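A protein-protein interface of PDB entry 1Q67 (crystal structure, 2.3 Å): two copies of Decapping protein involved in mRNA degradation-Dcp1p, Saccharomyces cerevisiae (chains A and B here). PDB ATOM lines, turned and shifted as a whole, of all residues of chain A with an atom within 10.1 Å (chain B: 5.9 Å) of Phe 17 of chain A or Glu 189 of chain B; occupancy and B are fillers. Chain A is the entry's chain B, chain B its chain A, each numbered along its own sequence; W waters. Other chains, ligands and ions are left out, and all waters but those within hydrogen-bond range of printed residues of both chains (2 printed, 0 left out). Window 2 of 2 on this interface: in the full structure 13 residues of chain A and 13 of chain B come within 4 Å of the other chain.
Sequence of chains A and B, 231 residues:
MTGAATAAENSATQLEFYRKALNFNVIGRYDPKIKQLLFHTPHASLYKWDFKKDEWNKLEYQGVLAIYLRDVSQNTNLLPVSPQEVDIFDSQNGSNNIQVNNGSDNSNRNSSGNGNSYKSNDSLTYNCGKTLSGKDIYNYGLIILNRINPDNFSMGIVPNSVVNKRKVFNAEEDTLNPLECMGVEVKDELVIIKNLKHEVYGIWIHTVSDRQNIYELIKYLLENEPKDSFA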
ATOM      1  N   PHE A  17     -11.236 -19.203  24.587  1.00  0.00           N
ATOM      2  CA  PHE A  17     -11.254 -18.756  23.163  1.00  0.00           C
ATOM      3  C   PHE A  17     -12.401 -19.423  22.407  1.00  0.00           C
ATOM      4  O   PHE A  17     -12.732 -20.586  22.657  1.00  0.00           O
ATOM      5  CB  PHE A  17      -9.925 -19.096  22.483  1.00  0.00           C
ATOM      6  CG  PHE A  17      -9.869 -18.703  21.033  1.00  0.00           C
ATOM      7  CD1 PHE A  17      -9.965 -17.365  20.655  1.00  0.00           C
ATOM      8  CD2 PHE A  17      -9.733 -19.672  20.039  1.00  0.00           C
ATOM      9  CE1 PHE A  17      -9.926 -16.998  19.308  1.00  0.00           C
ATOM     10  CE2 PHE A  17      -9.694 -19.317  18.692  1.00  0.00           C
ATOM     11  CZ  PHE A  17      -9.791 -17.975  18.325  1.00  0.00           C
ATOM     12  N   TYR A  18     -13.001 -18.682  21.481  1.00  0.00           N
ATOM     13  CA  TYR A  18     -14.114 -19.193  20.692  1.00  0.00           C
ATOM     14  C   TYR A  18     -13.959 -18.851  19.215  1.00  0.00           C
ATOM     15  O   TYR A  18     -13.616 -17.724  18.866  1.00  0.00           O
ATOM     16  CB  TYR A  18     -15.430 -18.609  21.205  1.00  0.00           C
ATOM     17  CG  TYR A  18     -15.799 -19.045  22.603  1.00  0.00           C
ATOM     18  CD1 TYR A  18     -16.099 -20.379  22.879  1.00  0.00           C
ATOM     19  CD2 TYR A  18     -15.863 -18.124  23.648  1.00  0.00           C
ATOM     20  CE1 TYR A  18     -16.457 -20.787  24.164  1.00  0.00           C
ATOM     21  CE2 TYR A  18     -16.220 -18.522  24.938  1.00  0.00           C
ATOM     22  CZ  TYR A  18     -16.516 -19.855  25.188  1.00  0.00           C
ATOM     23  OH  TYR A  18     -16.870 -20.256  26.458  1.00  0.00           O
ATOM     24  N   ARG A  19     -14.207 -19.831  18.352  1.00  0.00           N
ATOM     25  CA  ARG A  19     -14.117 -19.619  16.913  1.00  0.00           C
ATOM     26  C   ARG A  19     -15.259 -18.695  16.489  1.00  0.00           C
ATOM     27  O   ARG A  19     -16.392 -18.857  16.946  1.00  0.00           O
ATOM     28  CB  ARG A  19     -14.273 -20.947  16.170  1.00  0.00           C
ATOM     29  CG  ARG A  19     -13.366 -22.068  16.638  1.00  0.00           C
ATOM     30  CD  ARG A  19     -12.010 -22.023  15.954  1.00  0.00           C
ATOM     31  NE  ARG A  19     -11.439 -23.362  15.817  1.00  0.00           N
ATOM     32  CZ  ARG A  19     -12.031 -24.365  15.171  1.00  0.00           C
ATOM     33  NH1 ARG A  19     -13.218 -24.187  14.596  1.00  0.00           N
ATOM     34  NH2 ARG A  19     -11.438 -25.551  15.093  1.00  0.00           N
ATOM     35  N   LYS A  20     -14.964 -17.737  15.621  1.00  0.00           N
ATOM     36  CA  LYS A  20     -15.977 -16.810  15.124  1.00  0.00           C
ATOM     37  C   LYS A  20     -15.816 -16.530  13.633  1.00  0.00           C
ATOM     38  O   LYS A  20     -16.779 -16.182  12.946  1.00  0.00           O
ATOM     39  CB  LYS A  20     -15.912 -15.477  15.874  1.00  0.00           C
ATOM     40  CG  LYS A  20     -16.459 -15.520  17.285  1.00  0.00           C
ATOM     41  CD  LYS A  20     -16.678 -14.118  17.825  1.00  0.00           C
ATOM     42  CE  LYS A  20     -15.371 -13.365  17.975  1.00  0.00           C
ATOM     43  NZ  LYS A  20     -14.461 -14.068  18.909  1.00  0.00           N
ATOM     44  N   ALA A  21     -14.596 -16.693  13.134  1.00  0.00           N
ATOM     45  CA  ALA A  21     -14.301 -16.409  11.734  1.00  0.00           C
ATOM     46  C   ALA A  21     -14.942 -17.339  10.712  1.00  0.00           C
ATOM     47  O   ALA A  21     -15.195 -18.515  10.975  1.00  0.00           O
ATOM     48  CB  ALA A  21     -12.791 -16.383  11.523  1.00  0.00           C
ATOM     49  N   PRO A  42      -1.988 -12.223   9.484  1.00  0.00           N
ATOM     50  CA  PRO A  42      -2.891 -11.992  10.625  1.00  0.00           C
ATOM     51  C   PRO A  42      -2.824 -10.673  11.381  1.00  0.00           C
ATOM     52  O   PRO A  42      -3.860 -10.075  11.691  1.00  0.00           O
ATOM     53  CB  PRO A  42      -2.582 -13.167  11.567  1.00  0.00           C
ATOM     54  CG  PRO A  42      -1.918 -14.186  10.685  1.00  0.00           C
ATOM     55  CD  PRO A  42      -1.092 -13.359   9.756  1.00  0.00           C
ATOM     56  N   HIS A  43      -1.614 -10.224  11.692  1.00  0.00           N
ATOM     57  CA  HIS A  43      -1.460  -9.009  12.479  1.00  0.00           C
ATOM     58  C   HIS A  43      -0.466  -7.996  11.923  1.00  0.00           C
ATOM     59  O   HIS A  43       0.723  -8.286  11.792  1.00  0.00           O
ATOM     60  CB  HIS A  43      -1.052  -9.406  13.899  1.00  0.00           C
ATOM     61  CG  HIS A  43      -1.855 -10.543  14.454  1.00  0.00           C
ATOM     62  ND1 HIS A  43      -3.179 -10.413  14.819  1.00  0.00           N
ATOM     63  CD2 HIS A  43      -1.541 -11.848  14.641  1.00  0.00           C
ATOM     64  CE1 HIS A  43      -3.645 -11.587  15.206  1.00  0.00           C
ATOM     65  NE2 HIS A  43      -2.673 -12.476  15.107  1.00  0.00           N
ATOM     66  N   ARG A 147      -9.401  -5.632  13.415  1.00  0.00           N
ATOM     67  CA  ARG A 147     -10.015  -6.783  14.074  1.00  0.00           C
ATOM     68  C   ARG A 147     -10.890  -6.385  15.250  1.00  0.00           C
ATOM     69  O   ARG A 147     -11.913  -7.013  15.515  1.00  0.00           O
ATOM     70  CB  ARG A 147      -8.935  -7.726  14.609  1.00  0.00           C
ATOM     71  CG  ARG A 147      -8.236  -8.602  13.588  1.00  0.00           C
ATOM     72  CD  ARG A 147      -7.013  -9.247  14.233  1.00  0.00           C
ATOM     73  NE  ARG A 147      -6.420 -10.286  13.398  1.00  0.00           N
ATOM     74  CZ  ARG A 147      -6.937 -11.499  13.249  1.00  0.00           C
ATOM     75  NH1 ARG A 147      -8.055 -11.821  13.889  1.00  0.00           N
ATOM     76  NH2 ARG A 147      -6.344 -12.385  12.454  1.00  0.00           N
ATOM     77  N   ILE A 148     -10.469  -5.348  15.962  1.00  0.00           N
ATOM     78  CA  ILE A 148     -11.178  -4.886  17.149  1.00  0.00           C
ATOM     79  C   ILE A 148     -12.324  -3.918  16.867  1.00  0.00           C
ATOM     80  O   ILE A 148     -13.197  -3.731  17.713  1.00  0.00           O
ATOM     81  CB  ILE A 148     -10.179  -4.259  18.147  1.00  0.00           C
ATOM     82  CG1 ILE A 148      -8.966  -5.184  18.298  1.00  0.00           C
ATOM     83  CG2 ILE A 148     -10.840  -4.066  19.505  1.00  0.00           C
ATOM     84  CD1 ILE A 148      -9.314  -6.627  18.678  1.00  0.00           C
ATOM     85  N   ASN A 149     -12.311  -3.290  15.693  1.00  0.00           N
ATOM     86  CA  ASN A 149     -13.391  -2.391  15.288  1.00  0.00           C
ATOM     87  C   ASN A 149     -13.542  -2.530  13.779  1.00  0.00           C
ATOM     88  O   ASN A 149     -12.731  -3.190  13.134  1.00  0.00           O
ATOM     89  CB  ASN A 149     -13.126  -0.934  15.701  1.00  0.00           C
ATOM     90  CG  ASN A 149     -11.837  -0.372  15.137  1.00  0.00           C
ATOM     91  OD1 ASN A 149     -11.539  -0.528  13.953  1.00  0.00           O
ATOM     92  ND2 ASN A 149     -11.075   0.311  15.985  1.00  0.00           N
ATOM     93  N   VAL B 186     -11.597 -11.319  30.371  1.00  0.00           N
ATOM     94  CA  VAL B 186     -11.104 -11.642  29.050  1.00  0.00           C
ATOM     95  C   VAL B 186     -12.320 -11.822  28.165  1.00  0.00           C
ATOM     96  O   VAL B 186     -13.130 -12.722  28.388  1.00  0.00           O
ATOM     97  CB  VAL B 186     -10.281 -12.943  29.058  1.00  0.00           C
ATOM     98  CG1 VAL B 186     -10.021 -13.409  27.630  1.00  0.00           C
ATOM     99  CG2 VAL B 186      -8.970 -12.714  29.778  1.00  0.00           C
ATOM    100  N   LYS B 187     -12.465 -10.936  27.185  1.00  0.00           N
ATOM    101  CA  LYS B 187     -13.573 -11.003  26.244  1.00  0.00           C
ATOM    102  C   LYS B 187     -12.975 -10.980  24.843  1.00  0.00           C
ATOM    103  O   LYS B 187     -12.228 -10.062  24.488  1.00  0.00           O
ATOM    104  CB  LYS B 187     -14.525  -9.820  26.449  1.00  0.00           C
ATOM    105  CG  LYS B 187     -15.688  -9.804  25.475  1.00  0.00           C
ATOM    106  CD  LYS B 187     -16.768  -8.820  25.889  1.00  0.00           C
ATOM    107  CE  LYS B 187     -17.455  -9.272  27.165  1.00  0.00           C
ATOM    108  NZ  LYS B 187     -18.589  -8.377  27.516  1.00  0.00           N
ATOM    109  N   ASP B 188     -13.298 -11.997  24.054  1.00  0.00           N
ATOM    110  CA  ASP B 188     -12.759 -12.109  22.706  1.00  0.00           C
ATOM    111  C   ASP B 188     -11.261 -12.366  22.845  1.00  0.00           C
ATOM    112  O   ASP B 188     -10.849 -13.350  23.458  1.00  0.00           O
ATOM    113  CB  ASP B 188     -13.002 -10.817  21.911  1.00  0.00           C
ATOM    114  CG  ASP B 188     -14.470 -10.597  21.584  1.00  0.00           C
ATOM    115  OD1 ASP B 188     -14.815  -9.499  21.097  1.00  0.00           O
ATOM    116  OD2 ASP B 188     -15.280 -11.524  21.805  1.00  0.00           O
ATOM    117  N   GLU B 189     -10.454 -11.471  22.292  1.00  0.00           N
ATOM    118  CA  GLU B 189      -9.005 -11.612  22.355  1.00  0.00           C
ATOM    119  C   GLU B 189      -8.427 -10.558  23.299  1.00  0.00           C
ATOM    120  O   GLU B 189      -7.220 -10.510  23.518  1.00  0.00           O
ATOM    121  CB  GLU B 189      -8.401 -11.409  20.961  1.00  0.00           C
ATOM    122  CG  GLU B 189      -9.238 -11.954  19.799  1.00  0.00           C
ATOM    123  CD  GLU B 189      -9.255 -13.473  19.726  1.00  0.00           C
ATOM    124  OE1 GLU B 189      -8.164 -14.079  19.610  1.00  0.00           O
ATOM    125  OE2 GLU B 189     -10.361 -14.062  19.775  1.00  0.00           O
ATOM    126  N   LEU B 190      -9.298  -9.730  23.862  1.00  0.00           N
ATOM    127  CA  LEU B 190      -8.879  -8.648  24.746  1.00  0.00           C
ATOM    128  C   LEU B 190      -8.885  -8.891  26.257  1.00  0.00           C
ATOM    129  O   LEU B 190      -9.805  -9.500  26.805  1.00  0.00           O
ATOM    130  CB  LEU B 190      -9.748  -7.418  24.488  1.00  0.00           C
ATOM    131  CG  LEU B 190      -9.838  -6.809  23.089  1.00  0.00           C
ATOM    132  CD1 LEU B 190     -10.920  -5.738  23.095  1.00  0.00           C
ATOM    133  CD2 LEU B 190      -8.491  -6.218  22.682  1.00  0.00           C
ATOM    134  N   VAL B 191      -7.845  -8.402  26.927  1.00  0.00           N
ATOM    135  CA  VAL B 191      -7.785  -8.477  28.378  1.00  0.00           C
ATOM    136  C   VAL B 191      -8.393  -7.119  28.724  1.00  0.00           C
ATOM    137  O   VAL B 191      -7.806  -6.083  28.436  1.00  0.00           O
ATOM    138  CB  VAL B 191      -6.340  -8.550  28.904  1.00  0.00           C
ATOM    139  CG1 VAL B 191      -6.338  -8.409  30.429  1.00  0.00           C
ATOM    140  CG2 VAL B 191      -5.706  -9.878  28.504  1.00  0.00           C
ATOM    141  N   ILE B 203      -6.787  -4.516  26.137  1.00  0.00           N
ATOM    142  CA  ILE B 203      -5.427  -4.759  25.700  1.00  0.00           C
ATOM    143  C   ILE B 203      -5.323  -6.010  24.846  1.00  0.00           C
ATOM    144  O   ILE B 203      -5.691  -7.106  25.277  1.00  0.00           O
ATOM    145  CB  ILE B 203      -4.468  -4.906  26.900  1.00  0.00           C
ATOM    146  CG1 ILE B 203      -4.555  -3.670  27.797  1.00  0.00           C
ATOM    147  CG2 ILE B 203      -3.042  -5.091  26.395  1.00  0.00           C
ATOM    148  CD1 ILE B 203      -3.654  -3.725  29.034  1.00  0.00           C
ATOM    149  N   TRP B 204      -4.825  -5.844  23.627  1.00  0.00           N
ATOM    150  CA  TRP B 204      -4.657  -6.982  22.740  1.00  0.00           C
ATOM    151  C   TRP B 204      -3.230  -7.479  22.868  1.00  0.00           C
ATOM    152  O   TRP B 204      -2.276  -6.708  22.762  1.00  0.00           O
ATOM    153  CB  TRP B 204      -4.926  -6.613  21.281  1.00  0.00           C
ATOM    154  CG  TRP B 204      -4.916  -7.835  20.421  1.00  0.00           C
ATOM    155  CD1 TRP B 204      -5.918  -8.751  20.297  1.00  0.00           C
ATOM    156  CD2 TRP B 204      -3.810  -8.349  19.669  1.00  0.00           C
ATOM    157  NE1 TRP B 204      -5.506  -9.805  19.523  1.00  0.00           N
ATOM    158  CE2 TRP B 204      -4.216  -9.585  19.123  1.00  0.00           C
ATOM    159  CE3 TRP B 204      -2.514  -7.888  19.408  1.00  0.00           C
ATOM    160  CZ2 TRP B 204      -3.373 -10.370  18.329  1.00  0.00           C
ATOM    161  CZ3 TRP B 204      -1.671  -8.671  18.613  1.00  0.00           C
ATOM    162  CH2 TRP B 204      -2.108  -9.897  18.086  1.00  0.00           C
ATOM    163  N   ILE B 205      -3.094  -8.776  23.100  1.00  0.00           N
ATOM    164  CA  ILE B 205      -1.792  -9.404  23.256  1.00  0.00           C
ATOM    165  C   ILE B 205      -1.700 -10.555  22.251  1.00  0.00           C
ATOM    166  O   ILE B 205      -2.623 -11.356  22.148  1.00  0.00           O
ATOM    167  CB  ILE B 205      -1.631  -9.943  24.705  1.00  0.00           C
ATOM    168  CG1 ILE B 205      -1.678  -8.775  25.694  1.00  0.00           C
ATOM    169  CG2 ILE B 205      -0.327 -10.706  24.843  1.00  0.00           C
ATOM    170  CD1 ILE B 205      -1.697  -9.186  27.159  1.00  0.00           C
ATOM    171  N   ARG B 211      -1.618 -13.907  27.220  1.00  0.00           N
ATOM    172  CA  ARG B 211      -2.934 -13.341  27.453  1.00  0.00           C
ATOM    173  C   ARG B 211      -3.557 -13.919  28.712  1.00  0.00           C
ATOM    174  O   ARG B 211      -4.131 -13.195  29.526  1.00  0.00           O
ATOM    175  CB  ARG B 211      -3.840 -13.617  26.253  1.00  0.00           C
ATOM    176  CG  ARG B 211      -5.112 -12.797  26.230  1.00  0.00           C
ATOM    177  CD  ARG B 211      -5.943 -13.142  25.007  1.00  0.00           C
ATOM    178  NE  ARG B 211      -5.125 -13.166  23.797  1.00  0.00           N
ATOM    179  CZ  ARG B 211      -5.578 -13.506  22.593  1.00  0.00           C
ATOM    180  NH1 ARG B 211      -6.849 -13.852  22.431  1.00  0.00           N
ATOM    181  NH2 ARG B 211      -4.755 -13.515  21.555  1.00  0.00           N
HETATM  182  O   HOH W   1     -12.283 -12.206  19.071  1.00  0.00           O
HETATM  183  O   HOH W   2     -12.664 -15.870  22.128  1.00  0.00           O
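Among the printed residues, pairs that only touch across the chains: Phe 17 of chain A with Glu 189 of chain B, His 43 of chain A with Trp 204 of chain B and Ile 148 of chain A with Leu 190 of chain B.
Water W1 lies within hydrogen-bond range of OE2 of Glu 189 of chain B (2.8 Å) and NZ of Lys 20 of chain A (2.9 Å). Water W2 bridges the backbone NH (N) of Tyr 18 of chain A (2.9 Å) and the backbone carbonyl oxygen (O) of Asp 188 of chain B (3.4 Å).
Of the 10 printed residues of chain B, 4 touch a printed residue of chain A. Printed residues of chain B that touch a printed residue of chain A: Asp 188, Glu 189, Leu 190 and Trp 204. Among the printed residues, 4 pairs touch across the chains. Among the printed residues, Asp or Glu carboxylates within 4 Å of a Lys or Arg side-chain nitrogen of the other chain: Lys 20 of chain A with Asp 188 of chain B.
The side-chain carboxylate (OD2) of Asp 188 of chain B is in salt-bridge range of the side-chain amino group (NZ) of Lys 20 of chain A, at 3.9 Å.
Phe 17 of chain A touches one residue of chain B. Tyr 18 of chain A touches none of the printed residues of chain B. Arg 19 of chain A touches none of the printed residues of chain B. Of the printed residues of chain B, Lys 20 of chain A touches Asp 188. Printed residues of chain B within 4 Å of His 43 of chain A: Trp 204 (3.4 Å). Printed residues of chain B within 4 Å of Ile 148 of chain A: Leu 190 (3.96 Å). Of chain A, only Phe 17 comes within 4 Å of Glu 189 of chain B. Of the printed residues of chain A, Trp 204 of chain B touches His 43 (3.4 Å).
No position is printed for both chains.
The side-chain carboxylate (OE1) of Glu 189 of chain B is in salt-bridge range of the guanidinium group (NH1) of Arg 211 of chain B (3.1 Å).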
